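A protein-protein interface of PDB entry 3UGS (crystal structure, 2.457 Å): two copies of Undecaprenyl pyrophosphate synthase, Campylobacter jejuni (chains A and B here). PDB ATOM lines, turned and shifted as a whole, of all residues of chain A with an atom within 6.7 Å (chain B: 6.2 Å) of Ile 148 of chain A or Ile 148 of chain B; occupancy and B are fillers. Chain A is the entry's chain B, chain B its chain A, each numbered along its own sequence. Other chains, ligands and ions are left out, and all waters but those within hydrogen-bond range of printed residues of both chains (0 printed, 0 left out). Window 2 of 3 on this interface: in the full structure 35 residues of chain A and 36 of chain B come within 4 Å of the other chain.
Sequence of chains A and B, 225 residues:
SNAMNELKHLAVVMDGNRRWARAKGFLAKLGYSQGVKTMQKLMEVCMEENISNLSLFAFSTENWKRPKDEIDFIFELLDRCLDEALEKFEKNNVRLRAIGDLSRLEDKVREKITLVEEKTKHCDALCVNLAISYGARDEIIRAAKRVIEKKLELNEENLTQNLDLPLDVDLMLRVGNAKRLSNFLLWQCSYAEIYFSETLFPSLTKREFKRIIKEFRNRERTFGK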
ATOM      1  N   ALA A 143      11.183 -24.075 -22.580  1.00  0.00           N
ATOM      2  CA  ALA A 143      11.731 -23.182 -21.552  1.00  0.00           C
ATOM      3  C   ALA A 143      11.433 -23.723 -20.160  1.00  0.00           C
ATOM      4  O   ALA A 143      12.278 -23.669 -19.253  1.00  0.00           O
ATOM      5  CB  ALA A 143      11.188 -21.805 -21.689  1.00  0.00           C
ATOM      6  N   ALA A 144      10.224 -24.263 -20.014  1.00  0.00           N
ATOM      7  CA  ALA A 144       9.763 -24.845 -18.728  1.00  0.00           C
ATOM      8  C   ALA A 144      10.608 -26.091 -18.326  1.00  0.00           C
ATOM      9  O   ALA A 144      10.862 -26.347 -17.169  1.00  0.00           O
ATOM     10  CB  ALA A 144       8.291 -25.229 -18.783  1.00  0.00           C
ATOM     11  N   LYS A 145      10.994 -26.867 -19.312  1.00  0.00           N
ATOM     12  CA  LYS A 145      11.808 -28.055 -19.058  1.00  0.00           C
ATOM     13  C   LYS A 145      13.231 -27.666 -18.645  1.00  0.00           C
ATOM     14  O   LYS A 145      13.829 -28.302 -17.799  1.00  0.00           O
ATOM     15  CB  LYS A 145      11.842 -28.968 -20.268  1.00  0.00           C
ATOM     16  CG  LYS A 145      10.476 -29.529 -20.594  1.00  0.00           C
ATOM     17  CD  LYS A 145      10.483 -30.130 -21.984  1.00  0.00           C
ATOM     18  CE  LYS A 145       9.777 -31.476 -22.012  1.00  0.00           C
ATOM     19  NZ  LYS A 145      10.206 -32.190 -23.250  1.00  0.00           N
ATOM     20  N   ARG A 146      13.755 -26.636 -19.286  1.00  0.00           N
ATOM     21  CA  ARG A 146      15.076 -26.110 -18.947  1.00  0.00           C
ATOM     22  C   ARG A 146      15.139 -25.619 -17.487  1.00  0.00           C
ATOM     23  O   ARG A 146      16.157 -25.738 -16.791  1.00  0.00           O
ATOM     24  CB  ARG A 146      15.483 -24.946 -19.845  1.00  0.00           C
ATOM     25  CG  ARG A 146      15.866 -25.312 -21.250  1.00  0.00           C
ATOM     26  CD  ARG A 146      15.917 -24.033 -22.122  1.00  0.00           C
ATOM     27  NE  ARG A 146      16.433 -24.322 -23.449  1.00  0.00           N
ATOM     28  CZ  ARG A 146      16.097 -23.689 -24.562  1.00  0.00           C
ATOM     29  NH1 ARG A 146      15.233 -22.662 -24.542  1.00  0.00           N
ATOM     30  NH2 ARG A 146      16.630 -24.100 -25.704  1.00  0.00           N
ATOM     31  N   VAL A 147      14.036 -25.006 -17.081  1.00  0.00           N
ATOM     32  CA  VAL A 147      13.881 -24.475 -15.715  1.00  0.00           C
ATOM     33  C   VAL A 147      13.857 -25.632 -14.717  1.00  0.00           C
ATOM     34  O   VAL A 147      14.486 -25.606 -13.665  1.00  0.00           O
ATOM     35  CB  VAL A 147      12.610 -23.642 -15.537  1.00  0.00           C
ATOM     36  CG1 VAL A 147      12.330 -23.415 -14.057  1.00  0.00           C
ATOM     37  CG2 VAL A 147      12.754 -22.312 -16.269  1.00  0.00           C
ATOM     38  N   ILE A 148      13.090 -26.637 -15.080  1.00  0.00           N
ATOM     39  CA  ILE A 148      12.975 -27.882 -14.304  1.00  0.00           C
ATOM     40  C   ILE A 148      14.312 -28.641 -14.254  1.00  0.00           C
ATOM     41  O   ILE A 148      14.819 -28.987 -13.191  1.00  0.00           O
ATOM     42  CB  ILE A 148      11.875 -28.810 -14.839  1.00  0.00           C
ATOM     43  CG1 ILE A 148      10.517 -28.287 -14.346  1.00  0.00           C
ATOM     44  CG2 ILE A 148      12.070 -30.259 -14.368  1.00  0.00           C
ATOM     45  CD1 ILE A 148       9.344 -29.093 -14.868  1.00  0.00           C
ATOM     46  N   GLU A 149      14.895 -28.807 -15.416  1.00  0.00           N
ATOM     47  CA  GLU A 149      16.208 -29.452 -15.575  1.00  0.00           C
ATOM     48  C   GLU A 149      17.316 -28.751 -14.756  1.00  0.00           C
ATOM     49  O   GLU A 149      18.297 -29.372 -14.339  1.00  0.00           O
ATOM     50  CB  GLU A 149      16.610 -29.501 -17.046  1.00  0.00           C
ATOM     51  CG  GLU A 149      17.910 -30.243 -17.316  1.00  0.00           C
ATOM     52  CD  GLU A 149      18.280 -30.249 -18.802  1.00  0.00           C
ATOM     53  OE1 GLU A 149      17.505 -29.688 -19.632  1.00  0.00           O
ATOM     54  OE2 GLU A 149      19.347 -30.820 -19.146  1.00  0.00           O
ATOM     55  N   LYS A 150      17.126 -27.457 -14.530  1.00  0.00           N
ATOM     56  CA  LYS A 150      18.090 -26.628 -13.748  1.00  0.00           C
ATOM     57  C   LYS A 150      17.737 -26.531 -12.265  1.00  0.00           C
ATOM     58  O   LYS A 150      18.411 -25.866 -11.467  1.00  0.00           O
ATOM     59  CB  LYS A 150      18.206 -25.219 -14.320  1.00  0.00           C
ATOM     60  CG  LYS A 150      18.883 -25.156 -15.676  1.00  0.00           C
ATOM     61  CD  LYS A 150      18.958 -23.712 -16.148  1.00  0.00           C
ATOM     62  CE  LYS A 150      19.623 -23.563 -17.502  1.00  0.00           C
ATOM     63  NZ  LYS A 150      20.043 -22.150 -17.709  1.00  0.00           N
ATOM     64  N   LYS A 151      16.652 -27.185 -11.910  1.00  0.00           N
ATOM     65  CA  LYS A 151      16.200 -27.221 -10.499  1.00  0.00           C
ATOM     66  C   LYS A 151      15.803 -25.842  -9.989  1.00  0.00           C
ATOM     67  O   LYS A 151      15.847 -25.545  -8.815  1.00  0.00           O
ATOM     68  CB  LYS A 151      17.296 -27.776  -9.593  1.00  0.00           C
ATOM     69  CG  LYS A 151      17.613 -29.256  -9.801  1.00  0.00           C
ATOM     70  CD  LYS A 151      18.744 -29.669  -8.863  1.00  0.00           C
ATOM     71  CE  LYS A 151      19.144 -31.132  -9.011  1.00  0.00           C
ATOM     72  NZ  LYS A 151      20.184 -31.528  -8.004  1.00  0.00           N
ATOM     73  N   LEU A 152      15.419 -24.994 -10.916  1.00  0.00           N
ATOM     74  CA  LEU A 152      14.896 -23.658 -10.589  1.00  0.00           C
ATOM     75  C   LEU A 152      13.425 -23.732 -10.262  1.00  0.00           C
ATOM     76  O   LEU A 152      12.722 -24.645 -10.686  1.00  0.00           O
ATOM     77  CB  LEU A 152      15.099 -22.667 -11.736  1.00  0.00           C
ATOM     78  CG  LEU A 152      16.591 -22.397 -12.035  1.00  0.00           C
ATOM     79  CD1 LEU A 152      16.814 -21.577 -13.324  1.00  0.00           C
ATOM     80  CD2 LEU A 152      17.185 -21.705 -10.793  1.00  0.00           C
ATOM     81  N   LEU A 154       9.663 -22.796 -10.747  1.00  0.00           N
ATOM     82  CA  LEU A 154       8.867 -22.580 -11.947  1.00  0.00           C
ATOM     83  C   LEU A 154       8.009 -21.336 -11.752  1.00  0.00           C
ATOM     84  O   LEU A 154       6.968 -21.344 -11.147  1.00  0.00           O
ATOM     85  CB  LEU A 154       8.038 -23.806 -12.262  1.00  0.00           C
ATOM     86  CG  LEU A 154       7.419 -23.868 -13.655  1.00  0.00           C
ATOM     87  CD1 LEU A 154       8.428 -23.665 -14.794  1.00  0.00           C
ATOM     88  CD2 LEU A 154       6.696 -25.200 -13.850  1.00  0.00           C
ATOM     89  N   ALA B 143      -0.469 -23.590 -14.951  1.00  0.00           N
ATOM     90  CA  ALA B 143      -0.846 -24.779 -15.729  1.00  0.00           C
ATOM     91  C   ALA B 143       0.320 -25.775 -15.797  1.00  0.00           C
ATOM     92  O   ALA B 143       0.127 -26.957 -15.671  1.00  0.00           O
ATOM     93  CB  ALA B 143      -1.339 -24.431 -17.121  1.00  0.00           C
ATOM     94  N   ALA B 144       1.515 -25.257 -15.982  1.00  0.00           N
ATOM     95  CA  ALA B 144       2.761 -26.039 -16.004  1.00  0.00           C
ATOM     96  C   ALA B 144       2.965 -26.840 -14.736  1.00  0.00           C
ATOM     97  O   ALA B 144       3.412 -27.990 -14.752  1.00  0.00           O
ATOM     98  CB  ALA B 144       3.951 -25.138 -16.197  1.00  0.00           C
ATOM     99  N   LYS B 145       2.571 -26.222 -13.642  1.00  0.00           N
ATOM    100  CA  LYS B 145       2.685 -26.837 -12.319  1.00  0.00           C
ATOM    101  C   LYS B 145       1.663 -27.896 -12.051  1.00  0.00           C
ATOM    102  O   LYS B 145       1.953 -28.918 -11.423  1.00  0.00           O
ATOM    103  CB  LYS B 145       2.535 -25.775 -11.233  1.00  0.00           C
ATOM    104  CG  LYS B 145       3.810 -24.983 -11.067  1.00  0.00           C
ATOM    105  CD  LYS B 145       3.496 -23.646 -10.434  1.00  0.00           C
ATOM    106  CE  LYS B 145       4.631 -23.258  -9.504  1.00  0.00           C
ATOM    107  NZ  LYS B 145       4.482 -21.901  -8.918  1.00  0.00           N
ATOM    108  N   ARG B 146       0.450 -27.589 -12.481  1.00  0.00           N
ATOM    109  CA  ARG B 146      -0.662 -28.552 -12.433  1.00  0.00           C
ATOM    110  C   ARG B 146      -0.166 -29.825 -13.101  1.00  0.00           C
ATOM    111  O   ARG B 146      -0.391 -30.941 -12.646  1.00  0.00           O
ATOM    112  CB  ARG B 146      -1.905 -28.060 -13.138  1.00  0.00           C
ATOM    113  CG  ARG B 146      -2.734 -27.102 -12.287  1.00  0.00           C
ATOM    114  CD  ARG B 146      -3.644 -26.199 -13.120  1.00  0.00           C
ATOM    115  NE  ARG B 146      -4.566 -25.435 -12.305  1.00  0.00           N
ATOM    116  CZ  ARG B 146      -5.226 -24.352 -12.708  1.00  0.00           C
ATOM    117  NH1 ARG B 146      -5.076 -23.869 -13.933  1.00  0.00           N
ATOM    118  NH2 ARG B 146      -6.022 -23.714 -11.874  1.00  0.00           N
ATOM    119  N   VAL B 147       0.542 -29.614 -14.177  1.00  0.00           N
ATOM    120  CA  VAL B 147       1.028 -30.725 -14.995  1.00  0.00           C
ATOM    121  C   VAL B 147       2.049 -31.534 -14.225  1.00  0.00           C
ATOM    122  O   VAL B 147       2.035 -32.767 -14.255  1.00  0.00           O
ATOM    123  CB  VAL B 147       1.672 -30.299 -16.332  1.00  0.00           C
ATOM    124  CG1 VAL B 147       2.326 -31.512 -17.007  1.00  0.00           C
ATOM    125  CG2 VAL B 147       0.626 -29.676 -17.243  1.00  0.00           C
ATOM    126  N   ILE B 148       2.931 -30.804 -13.561  1.00  0.00           N
ATOM    127  CA  ILE B 148       4.047 -31.416 -12.789  1.00  0.00           C
ATOM    128  C   ILE B 148       3.538 -32.262 -11.603  1.00  0.00           C
ATOM    129  O   ILE B 148       4.028 -33.387 -11.321  1.00  0.00           O
ATOM    130  CB  ILE B 148       5.068 -30.378 -12.231  1.00  0.00           C
ATOM    131  CG1 ILE B 148       5.887 -29.753 -13.382  1.00  0.00           C
ATOM    132  CG2 ILE B 148       5.984 -31.028 -11.162  1.00  0.00           C
ATOM    133  CD1 ILE B 148       6.227 -30.747 -14.460  1.00  0.00           C
ATOM    134  N   GLU B 149       2.554 -31.699 -10.932  1.00  0.00           N
ATOM    135  CA  GLU B 149       1.985 -32.305  -9.711  1.00  0.00           C
ATOM    136  C   GLU B 149       1.040 -33.466 -10.004  1.00  0.00           C
ATOM    137  O   GLU B 149       0.624 -34.186  -9.110  1.00  0.00           O
ATOM    138  CB  GLU B 149       1.320 -31.261  -8.797  1.00  0.00           C
ATOM    139  CG  GLU B 149      -0.136 -30.948  -9.054  1.00  0.00           C
ATOM    140  CD  GLU B 149      -0.499 -29.493  -8.659  1.00  0.00           C
ATOM    141  OE1 GLU B 149       0.439 -28.680  -8.448  1.00  0.00           O
ATOM    142  OE2 GLU B 149      -1.706 -29.119  -8.600  1.00  0.00           O
ATOM    143  N   LYS B 150       0.669 -33.606 -11.264  1.00  0.00           N
ATOM    144  CA  LYS B 150      -0.035 -34.804 -11.738  1.00  0.00           C
ATOM    145  C   LYS B 150       0.922 -35.844 -12.315  1.00  0.00           C
ATOM    146  O   LYS B 150       0.529 -36.933 -12.715  1.00  0.00           O
ATOM    147  CB  LYS B 150      -1.077 -34.476 -12.775  1.00  0.00           C
ATOM    148  CG  LYS B 150      -2.218 -33.639 -12.251  1.00  0.00           C
ATOM    149  CD  LYS B 150      -3.220 -33.356 -13.366  1.00  0.00           C
ATOM    150  CE  LYS B 150      -4.310 -32.421 -12.874  1.00  0.00           C
ATOM    151  NZ  LYS B 150      -5.376 -32.320 -13.877  1.00  0.00           N
ATOM    152  N   LYS B 151       2.179 -35.467 -12.378  1.00  0.00           N
ATOM    153  CA  LYS B 151       3.249 -36.370 -12.840  1.00  0.00           C
ATOM    154  C   LYS B 151       3.097 -36.704 -14.304  1.00  0.00           C
ATOM    155  O   LYS B 151       3.446 -37.781 -14.765  1.00  0.00           O
ATOM    156  CB  LYS B 151       3.293 -37.634 -11.998  1.00  0.00           C
ATOM    157  CG  LYS B 151       3.465 -37.337 -10.511  1.00  0.00           C
ATOM    158  CD  LYS B 151       3.283 -38.567  -9.630  1.00  0.00           C
ATOM    159  CE  LYS B 151       3.238 -38.190  -8.139  1.00  0.00           C
ATOM    160  NZ  LYS B 151       2.052 -37.352  -7.743  1.00  0.00           N
ATOM    161  N   LEU B 152       2.600 -35.706 -15.021  1.00  0.00           N
ATOM    162  CA  LEU B 152       2.411 -35.760 -16.480  1.00  0.00           C
ATOM    163  C   LEU B 152       3.621 -35.198 -17.229  1.00  0.00           C
ATOM    164  O   LEU B 152       4.324 -34.300 -16.744  1.00  0.00           O
ATOM    165  CB  LEU B 152       1.150 -35.000 -16.909  1.00  0.00           C
ATOM    166  CG  LEU B 152      -0.200 -35.444 -16.343  1.00  0.00           C
ATOM    167  CD1 LEU B 152      -1.338 -34.440 -16.624  1.00  0.00           C
ATOM    168  CD2 LEU B 152      -0.552 -36.794 -16.943  1.00  0.00           C
ATOM    169  N   LEU B 154       5.423 -32.836 -19.542  1.00  0.00           N
ATOM    170  CA  LEU B 154       5.300 -31.450 -20.048  1.00  0.00           C
ATOM    171  C   LEU B 154       5.307 -31.453 -21.572  1.00  0.00           C
ATOM    172  O   LEU B 154       6.314 -31.738 -22.200  1.00  0.00           O
ATOM    173  CB  LEU B 154       6.418 -30.501 -19.566  1.00  0.00           C
ATOM    174  CG  LEU B 154       6.150 -29.667 -18.313  1.00  0.00           C
ATOM    175  CD1 LEU B 154       7.419 -28.956 -17.821  1.00  0.00           C
ATOM    176  CD2 LEU B 154       5.001 -28.682 -18.550  1.00  0.00           C
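Leu 154 of chain B touches Ala 144 of chain A (CD1 to CB, 3.9 Å). Leu 154 of chain B touches Lys 145 of chain A. Ile 148 of chain A touches Ile 148 of chain B (CD1 to CD1, 3.6 Å). Ile 148 of chain A touches Leu 154 of chain B (CD1 to CD1, 3.5 Å). CD2 of Leu 154 of chain A touches CB of Ala 144 of chain B (3.6 Å).
Ala 144 of chain A touches Leu 154 of chain B, and with the chains exchanged Leu 154 of chain A touches Ala 144 of chain B. Lys 145 of chain A touches Leu 154 of chain B, and with the chains exchanged Leu 154 of chain A touches Lys 145 of chain B. Ile 148 of chain A touches its own counterpart, Ile 148 of chain B. Ile 148 of chain A touches Leu 154 of chain B, but with the chains exchanged Leu 154 of chain A does not touch Ile 148 of chain B (4.6 Å). Positions printed for both chains: 143, 144, 145, 146, 147, 148, 149, 150, 151, 152 and 154. Of the 6 pairs that touch across the chains among the printed residues, 5 have their exchanged pair printed and touching as well.
O of Leu 154 of chain A lies within hydrogen-bond range of NZ of Lys 145 of chain B (3.4 Å).
Of the printed residues of chain B, Ala 144 of chain A touches Leu 154. Val 147 of chain A touches none of the printed residues of chain B. Ile 148 of chain A touches just these residues of chain B: Ile 148 (3.6 Å) and Leu 154 (3.5 Å). Of the printed residues of chain A, Ala 144 of chain B touches Leu 154. Ile 148 of chain B touches just one residue of chain A: Ile 148 (3.6 Å). The nearest residue of chain B that does not touch Ile 148 of chain A is Ala 144 of chain B (6.0 Å).
Of the 11 printed residues of chain B, 4 touch a printed residue of chain A. Hydrophobic or aromatic side chains of chain B within 4 Å of the printed part of chain A: Ala 144, Ile 148 and Leu 154. Of the 11 printed residues of chain A, 4 touch a printed residue of chain B. Printed residues of chain A that touch a printed residue of chain B: Ala 144, Lys 145, Ile 148 and Leu 154. Among the printed residues, 6 pairs touch across the chains. Among the printed residues, no Asp or Glu carboxylate lies within 4 Å of a Lys or Arg side-chain nitrogen of the other chain.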
